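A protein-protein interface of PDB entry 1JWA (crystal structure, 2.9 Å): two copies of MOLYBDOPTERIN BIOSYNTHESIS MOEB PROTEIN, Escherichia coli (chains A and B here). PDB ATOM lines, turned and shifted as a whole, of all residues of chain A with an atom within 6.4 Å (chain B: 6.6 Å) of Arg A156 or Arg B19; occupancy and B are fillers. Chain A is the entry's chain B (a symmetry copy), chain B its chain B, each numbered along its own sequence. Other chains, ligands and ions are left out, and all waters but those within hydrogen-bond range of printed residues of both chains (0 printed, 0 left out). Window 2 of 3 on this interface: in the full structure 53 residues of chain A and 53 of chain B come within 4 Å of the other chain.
O of Arg B19 lies within hydrogen-bond range of OH of Tyr B215, at 2.6 Å.
The backbone carbonyl oxygen (O) of Met A157 lies within hydrogen-bond range of the backbone NH (N) of Ala A228 (3.1 Å).
The backbone NH (N) of Arg A156 lies within hydrogen-bond range of the backbone carbonyl oxygen (O) of Gly A191 (2.9 Å).
N of Met A193 is in hydrogen-bond range of O of Arg A156 (3.3 Å).
Among the printed residues, pairs that only touch across the chains: Arg A156 with Leu B18 (3.7 Å), Arg A156 with Arg B19 (3.6 Å), Met A157 with Tyr B215 (3.96 Å), Glu A189 with Ile B17 (3.9 Å), Ala A190 with Ile B17 (3.7 Å), Ala A190 with Arg B19 (3.8 Å), Gly A191 with Ile B17 (3.5 Å), Gly A191 with Leu B18 (3.4 Å), Val A192 with Leu B18 (3.4 Å), Met A193 with Gln B15 (3.8 Å), Met A193 with Leu B18 (3.3 Å), Met A193 with Met B206 (3.7 Å), Leu A196 with Met B206 (3.5 Å) and Met A229 with Tyr B215 (3.3 Å).
Arg A156 touches just these residues of chain B: Leu B18 and Arg B19.
Printed residues of chain B within 4 Å of Ala A190: Ile B17 and Arg B19.
Printed residues of chain B within 4 Å of Met A229: Tyr B215.
Of the printed residues of chain A, Ile B17 touches Glu A189, Ala A190 and Gly A191.
Of the printed residues of chain A, Leu B18 touches Arg A156, Gly A191, Val A192 and Met A193.
Of chain A, only Arg A156 (3.6 Å) and Ala A190 (3.8 Å) come within 4 Å of Arg B19.
Of the printed residues of chain A, Met B206 touches Met A193 and Leu A196.
The nearest residue of chain B that does not touch Arg A156 is Met B206 (6.1 Å).
The nearest residue of chain A that does not touch Arg B19 is Glu A189 (4.4 Å).
Hydrophobic or aromatic side chains of chain A that line the printed part of chain B: Met A157, Ala A190, Met A193, Leu A196 and Met A229.
Printed residues of chain B that touch a printed residue of chain A: Gln B15, Ile B17, Leu B18, Arg B19, Met B206 and Tyr B215.
Among the printed residues, no Asp or Glu carboxylate lies within 4 Å of a Lys or Arg side-chain nitrogen of the other chain.
No position is printed for both chains.
Of the 14 pairs that touch across the chains among the printed residues, none has its exchanged pair printed and touching as well.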
ATOM      1  N   ALA A 154     -19.687  -2.803 -22.306  1.00  0.00           N
ATOM      2  CA  ALA A 154     -18.769  -1.832 -21.733  1.00  0.00           C
ATOM      3  C   ALA A 154     -18.629  -0.594 -22.580  1.00  0.00           C
ATOM      4  O   ALA A 154     -18.662  -0.668 -23.773  1.00  0.00           O
ATOM      5  CB  ALA A 154     -17.417  -2.461 -21.536  1.00  0.00           C
ATOM      6  N   ILE A 155     -18.459   0.548 -21.953  1.00  0.00           N
ATOM      7  CA  ILE A 155     -18.269   1.781 -22.684  1.00  0.00           C
ATOM      8  C   ILE A 155     -17.729   2.789 -21.694  1.00  0.00           C
ATOM      9  O   ILE A 155     -18.010   2.681 -20.519  1.00  0.00           O
ATOM     10  CB  ILE A 155     -19.562   2.285 -23.301  1.00  0.00           C
ATOM     11  CG1 ILE A 155     -19.244   3.276 -24.413  1.00  0.00           C
ATOM     12  CG2 ILE A 155     -20.394   2.969 -22.292  1.00  0.00           C
ATOM     13  CD1 ILE A 155     -20.181   3.160 -25.583  1.00  0.00           C
ATOM     14  N   ARG A 156     -16.923   3.737 -22.172  1.00  0.00           N
ATOM     15  CA  ARG A 156     -16.351   4.754 -21.284  1.00  0.00           C
ATOM     16  C   ARG A 156     -15.579   4.131 -20.097  1.00  0.00           C
ATOM     17  O   ARG A 156     -14.448   3.678 -20.275  1.00  0.00           O
ATOM     18  CB  ARG A 156     -17.457   5.670 -20.778  1.00  0.00           C
ATOM     19  CG  ARG A 156     -17.891   6.698 -21.739  1.00  0.00           C
ATOM     20  CD  ARG A 156     -19.083   7.502 -21.295  1.00  0.00           C
ATOM     21  NE  ARG A 156     -20.175   7.496 -22.290  1.00  0.00           N
ATOM     22  CZ  ARG A 156     -21.378   6.991 -22.045  1.00  0.00           C
ATOM     23  NH1 ARG A 156     -21.640   6.476 -20.828  1.00  0.00           N
ATOM     24  NH2 ARG A 156     -22.311   7.003 -23.007  1.00  0.00           N
ATOM     25  N   MET A 157     -16.181   4.109 -18.913  1.00  0.00           N
ATOM     26  CA  MET A 157     -15.544   3.513 -17.758  1.00  0.00           C
ATOM     27  C   MET A 157     -16.569   2.647 -17.020  1.00  0.00           C
ATOM     28  O   MET A 157     -16.552   2.538 -15.805  1.00  0.00           O
ATOM     29  CB  MET A 157     -15.001   4.597 -16.822  1.00  0.00           C
ATOM     30  CG  MET A 157     -13.827   5.435 -17.341  1.00  0.00           C
ATOM     31  SD  MET A 157     -12.197   4.646 -17.226  1.00  0.00           S
ATOM     32  CE  MET A 157     -11.957   4.647 -15.592  1.00  0.00           C
ATOM     33  N   GLU A 158     -17.463   2.011 -17.756  1.00  0.00           N
ATOM     34  CA  GLU A 158     -18.501   1.235 -17.122  1.00  0.00           C
ATOM     35  C   GLU A 158     -18.806  -0.100 -17.827  1.00  0.00           C
ATOM     36  O   GLU A 158     -18.955  -0.166 -19.032  1.00  0.00           O
ATOM     37  CB  GLU A 158     -19.759   2.073 -17.066  1.00  0.00           C
ATOM     38  CG  GLU A 158     -20.835   1.462 -16.191  1.00  0.00           C
ATOM     39  CD  GLU A 158     -22.224   1.918 -16.573  1.00  0.00           C
ATOM     40  OE1 GLU A 158     -22.316   2.852 -17.428  1.00  0.00           O
ATOM     41  OE2 GLU A 158     -23.193   1.310 -16.018  1.00  0.00           O
ATOM     42  N   GLU A 189     -18.253   9.533 -30.913  1.00  0.00           N
ATOM     43  CA  GLU A 189     -18.689   8.390 -30.099  1.00  0.00           C
ATOM     44  C   GLU A 189     -18.371   8.614 -28.607  1.00  0.00           C
ATOM     45  O   GLU A 189     -18.127   9.753 -28.190  1.00  0.00           O
ATOM     46  CB  GLU A 189     -18.021   7.111 -30.608  1.00  0.00           C
ATOM     47  N   ALA A 190     -18.393   7.541 -27.811  1.00  0.00           N
ATOM     48  CA  ALA A 190     -17.991   7.608 -26.417  1.00  0.00           C
ATOM     49  C   ALA A 190     -16.656   6.858 -26.336  1.00  0.00           C
ATOM     50  O   ALA A 190     -16.448   5.858 -27.000  1.00  0.00           O
ATOM     51  CB  ALA A 190     -19.005   6.974 -25.542  1.00  0.00           C
ATOM     52  N   GLY A 191     -15.718   7.353 -25.560  1.00  0.00           N
ATOM     53  CA  GLY A 191     -14.470   6.651 -25.519  1.00  0.00           C
ATOM     54  C   GLY A 191     -14.619   5.324 -24.844  1.00  0.00           C
ATOM     55  O   GLY A 191     -15.721   4.844 -24.581  1.00  0.00           O
ATOM     56  N   VAL A 192     -13.473   4.771 -24.472  1.00  0.00           N
ATOM     57  CA  VAL A 192     -13.419   3.537 -23.681  1.00  0.00           C
ATOM     58  C   VAL A 192     -11.961   3.199 -23.268  1.00  0.00           C
ATOM     59  O   VAL A 192     -11.108   2.966 -24.140  1.00  0.00           O
ATOM     60  CB  VAL A 192     -14.088   2.373 -24.432  1.00  0.00           C
ATOM     61  CG1 VAL A 192     -13.500   2.240 -25.788  1.00  0.00           C
ATOM     62  CG2 VAL A 192     -13.995   1.069 -23.684  1.00  0.00           C
ATOM     63  N   MET A 193     -11.687   3.179 -21.954  1.00  0.00           N
ATOM     64  CA  MET A 193     -10.354   2.830 -21.410  1.00  0.00           C
ATOM     65  C   MET A 193     -10.012   1.355 -21.732  1.00  0.00           C
ATOM     66  O   MET A 193     -10.797   0.456 -21.511  1.00  0.00           O
ATOM     67  CB  MET A 193     -10.365   3.088 -19.918  1.00  0.00           C
ATOM     68  CG  MET A 193      -9.024   3.221 -19.261  1.00  0.00           C
ATOM     69  SD  MET A 193      -7.972   4.457 -20.003  1.00  0.00           S
ATOM     70  CE  MET A 193      -8.997   5.871 -19.861  1.00  0.00           C
ATOM     71  N   LEU A 196     -10.773  -1.793 -19.401  1.00  0.00           N
ATOM     72  CA  LEU A 196     -12.180  -2.070 -18.983  1.00  0.00           C
ATOM     73  C   LEU A 196     -12.798  -3.227 -19.748  1.00  0.00           C
ATOM     74  O   LEU A 196     -13.579  -4.023 -19.259  1.00  0.00           O
ATOM     75  CB  LEU A 196     -13.044  -0.818 -19.161  1.00  0.00           C
ATOM     76  CG  LEU A 196     -14.560  -0.934 -19.037  1.00  0.00           C
ATOM     77  CD1 LEU A 196     -15.010  -0.724 -17.622  1.00  0.00           C
ATOM     78  CD2 LEU A 196     -15.268   0.056 -19.942  1.00  0.00           C
ATOM     79  N   ALA A 228     -15.497   1.634 -13.061  1.00  0.00           N
ATOM     80  CA  ALA A 228     -14.046   1.833 -13.145  1.00  0.00           C
ATOM     81  C   ALA A 228     -13.604   3.119 -12.491  1.00  0.00           C
ATOM     82  O   ALA A 228     -12.658   3.155 -11.772  1.00  0.00           O
ATOM     83  CB  ALA A 228     -13.610   1.818 -14.599  1.00  0.00           C
ATOM     84  N   MET A 229     -14.304   4.197 -12.742  1.00  0.00           N
ATOM     85  CA  MET A 229     -13.898   5.459 -12.177  1.00  0.00           C
ATOM     86  C   MET A 229     -13.638   5.310 -10.697  1.00  0.00           C
ATOM     87  O   MET A 229     -12.704   5.926 -10.215  1.00  0.00           O
ATOM     88  CB  MET A 229     -14.970   6.518 -12.422  1.00  0.00           C
ATOM     89  CG  MET A 229     -14.437   7.911 -12.698  1.00  0.00           C
ATOM     90  SD  MET A 229     -13.085   7.952 -13.886  1.00  0.00           S
ATOM     91  CE  MET A 229     -13.621   9.156 -14.897  1.00  0.00           C
ATOM     92  N   GLN B  15      -9.579   6.693 -26.422  1.00  0.00           N
ATOM     93  CA  GLN B  15      -9.157   7.043 -25.082  1.00  0.00           C
ATOM     94  C   GLN B  15      -9.169   8.550 -24.947  1.00  0.00           C
ATOM     95  O   GLN B  15      -9.748   9.085 -24.011  1.00  0.00           O
ATOM     96  CB  GLN B  15      -7.777   6.476 -24.785  1.00  0.00           C
ATOM     97  CG  GLN B  15      -7.779   5.412 -23.643  1.00  0.00           C
ATOM     98  CD  GLN B  15      -6.739   4.291 -23.819  1.00  0.00           C
ATOM     99  OE1 GLN B  15      -5.629   4.510 -24.285  1.00  0.00           O
ATOM    100  NE2 GLN B  15      -7.104   3.108 -23.451  1.00  0.00           N
ATOM    101  N   ILE B  16      -8.564   9.221 -25.923  1.00  0.00           N
ATOM    102  CA  ILE B  16      -8.512  10.672 -25.910  1.00  0.00           C
ATOM    103  C   ILE B  16      -9.860  11.337 -25.779  1.00  0.00           C
ATOM    104  O   ILE B  16      -9.959  12.350 -25.108  1.00  0.00           O
ATOM    105  CB  ILE B  16      -7.855  11.226 -27.177  1.00  0.00           C
ATOM    106  CG1 ILE B  16      -6.329  11.098 -27.105  1.00  0.00           C
ATOM    107  CG2 ILE B  16      -8.229  12.713 -27.356  1.00  0.00           C
ATOM    108  CD1 ILE B  16      -5.676  10.746 -28.422  1.00  0.00           C
ATOM    109  N   ILE B  17     -10.884  10.804 -26.420  1.00  0.00           N
ATOM    110  CA  ILE B  17     -12.201  11.451 -26.353  1.00  0.00           C
ATOM    111  C   ILE B  17     -12.951  11.238 -25.077  1.00  0.00           C
ATOM    112  O   ILE B  17     -14.078  11.686 -24.998  1.00  0.00           O
ATOM    113  CB  ILE B  17     -13.126  11.015 -27.491  1.00  0.00           C
ATOM    114  CG1 ILE B  17     -13.168   9.500 -27.577  1.00  0.00           C
ATOM    115  CG2 ILE B  17     -12.597  11.529 -28.804  1.00  0.00           C
ATOM    116  CD1 ILE B  17     -14.339   8.977 -28.301  1.00  0.00           C
ATOM    117  N   LEU B  18     -12.371  10.520 -24.117  1.00  0.00           N
ATOM    118  CA  LEU B  18     -13.043  10.258 -22.843  1.00  0.00           C
ATOM    119  C   LEU B  18     -12.985  11.532 -22.054  1.00  0.00           C
ATOM    120  O   LEU B  18     -11.911  12.075 -21.809  1.00  0.00           O
ATOM    121  CB  LEU B  18     -12.330   9.176 -22.038  1.00  0.00           C
ATOM    122  CG  LEU B  18     -12.484   7.747 -22.497  1.00  0.00           C
ATOM    123  CD1 LEU B  18     -11.424   6.871 -21.856  1.00  0.00           C
ATOM    124  CD2 LEU B  18     -13.850   7.277 -22.152  1.00  0.00           C
ATOM    125  N   ARG B  19     -14.142  12.000 -21.624  1.00  0.00           N
ATOM    126  CA  ARG B  19     -14.209  13.258 -20.861  1.00  0.00           C
ATOM    127  C   ARG B  19     -13.336  13.146 -19.612  1.00  0.00           C
ATOM    128  O   ARG B  19     -13.423  12.177 -18.890  1.00  0.00           O
ATOM    129  CB  ARG B  19     -15.662  13.629 -20.505  1.00  0.00           C
ATOM    130  CG  ARG B  19     -16.705  12.539 -20.804  1.00  0.00           C
ATOM    131  CD  ARG B  19     -17.673  12.898 -21.974  1.00  0.00           C
ATOM    132  NE  ARG B  19     -18.147  11.704 -22.683  1.00  0.00           N
ATOM    133  CZ  ARG B  19     -19.183  11.662 -23.519  1.00  0.00           C
ATOM    134  NH1 ARG B  19     -19.883  12.756 -23.777  1.00  0.00           N
ATOM    135  NH2 ARG B  19     -19.513  10.508 -24.102  1.00  0.00           N
ATOM    136  N   GLY B  20     -12.473  14.134 -19.408  1.00  0.00           N
ATOM    137  CA  GLY B  20     -11.580  14.170 -18.278  1.00  0.00           C
ATOM    138  C   GLY B  20     -10.208  13.629 -18.608  1.00  0.00           C
ATOM    139  O   GLY B  20      -9.263  13.807 -17.851  1.00  0.00           O
ATOM    140  N   PHE B  21     -10.099  12.895 -19.705  1.00  0.00           N
ATOM    141  CA  PHE B  21      -8.841  12.302 -20.068  1.00  0.00           C
ATOM    142  C   PHE B  21      -8.233  13.224 -21.103  1.00  0.00           C
ATOM    143  O   PHE B  21      -7.236  13.844 -20.841  1.00  0.00           O
ATOM    144  CB  PHE B  21      -9.035  10.873 -20.588  1.00  0.00           C
ATOM    145  CG  PHE B  21      -7.768  10.037 -20.576  1.00  0.00           C
ATOM    146  CD1 PHE B  21      -7.178   9.645 -19.386  1.00  0.00           C
ATOM    147  CD2 PHE B  21      -7.163   9.639 -21.764  1.00  0.00           C
ATOM    148  CE1 PHE B  21      -5.979   8.869 -19.397  1.00  0.00           C
ATOM    149  CE2 PHE B  21      -5.986   8.890 -21.765  1.00  0.00           C
ATOM    150  CZ  PHE B  21      -5.416   8.500 -20.587  1.00  0.00           C
ATOM    151  N   ASP B  22      -8.794  13.255 -22.302  1.00  0.00           N
ATOM    152  CA  ASP B  22      -8.315  14.129 -23.362  1.00  0.00           C
ATOM    153  C   ASP B  22      -6.853  13.942 -23.711  1.00  0.00           C
ATOM    154  O   ASP B  22      -6.149  13.144 -23.120  1.00  0.00           O
ATOM    155  CB  ASP B  22      -8.511  15.549 -22.879  1.00  0.00           C
ATOM    156  CG  ASP B  22      -8.809  16.530 -23.970  1.00  0.00           C
ATOM    157  OD1 ASP B  22      -9.161  16.114 -25.087  1.00  0.00           O
ATOM    158  OD2 ASP B  22      -8.699  17.759 -23.735  1.00  0.00           O
ATOM    159  N   MET B 206      -5.823  -1.136 -15.062  1.00  0.00           N
ATOM    160  CA  MET B 206      -6.749  -0.015 -14.977  1.00  0.00           C
ATOM    161  C   MET B 206      -6.271   0.979 -13.918  1.00  0.00           C
ATOM    162  O   MET B 206      -6.036   2.155 -14.160  1.00  0.00           O
ATOM    163  CB  MET B 206      -8.107  -0.554 -14.571  1.00  0.00           C
ATOM    164  CG  MET B 206      -9.210   0.498 -14.421  1.00  0.00           C
ATOM    165  SD  MET B 206      -9.368   1.552 -15.777  1.00  0.00           S
ATOM    166  CE  MET B 206     -10.388   0.671 -16.888  1.00  0.00           C
ATOM    167  N   TYR B 215      -6.649  10.317 -13.328  1.00  0.00           N
ATOM    168  CA  TYR B 215      -8.029  10.131 -13.778  1.00  0.00           C
ATOM    169  C   TYR B 215      -8.702   9.264 -12.773  1.00  0.00           C
ATOM    170  O   TYR B 215      -8.102   8.307 -12.317  1.00  0.00           O
ATOM    171  CB  TYR B 215      -8.034   9.400 -15.083  1.00  0.00           C
ATOM    172  CG  TYR B 215      -9.324   9.494 -15.904  1.00  0.00           C
ATOM    173  CD1 TYR B 215      -9.906  10.715 -16.191  1.00  0.00           C
ATOM    174  CD2 TYR B 215      -9.902   8.348 -16.470  1.00  0.00           C
ATOM    175  CE1 TYR B 215     -11.045  10.789 -16.966  1.00  0.00           C
ATOM    176  CE2 TYR B 215     -11.012   8.427 -17.236  1.00  0.00           C
ATOM    177  CZ  TYR B 215     -11.587   9.644 -17.489  1.00  0.00           C
ATOM    178  OH  TYR B 215     -12.720   9.722 -18.262  1.00  0.00           O
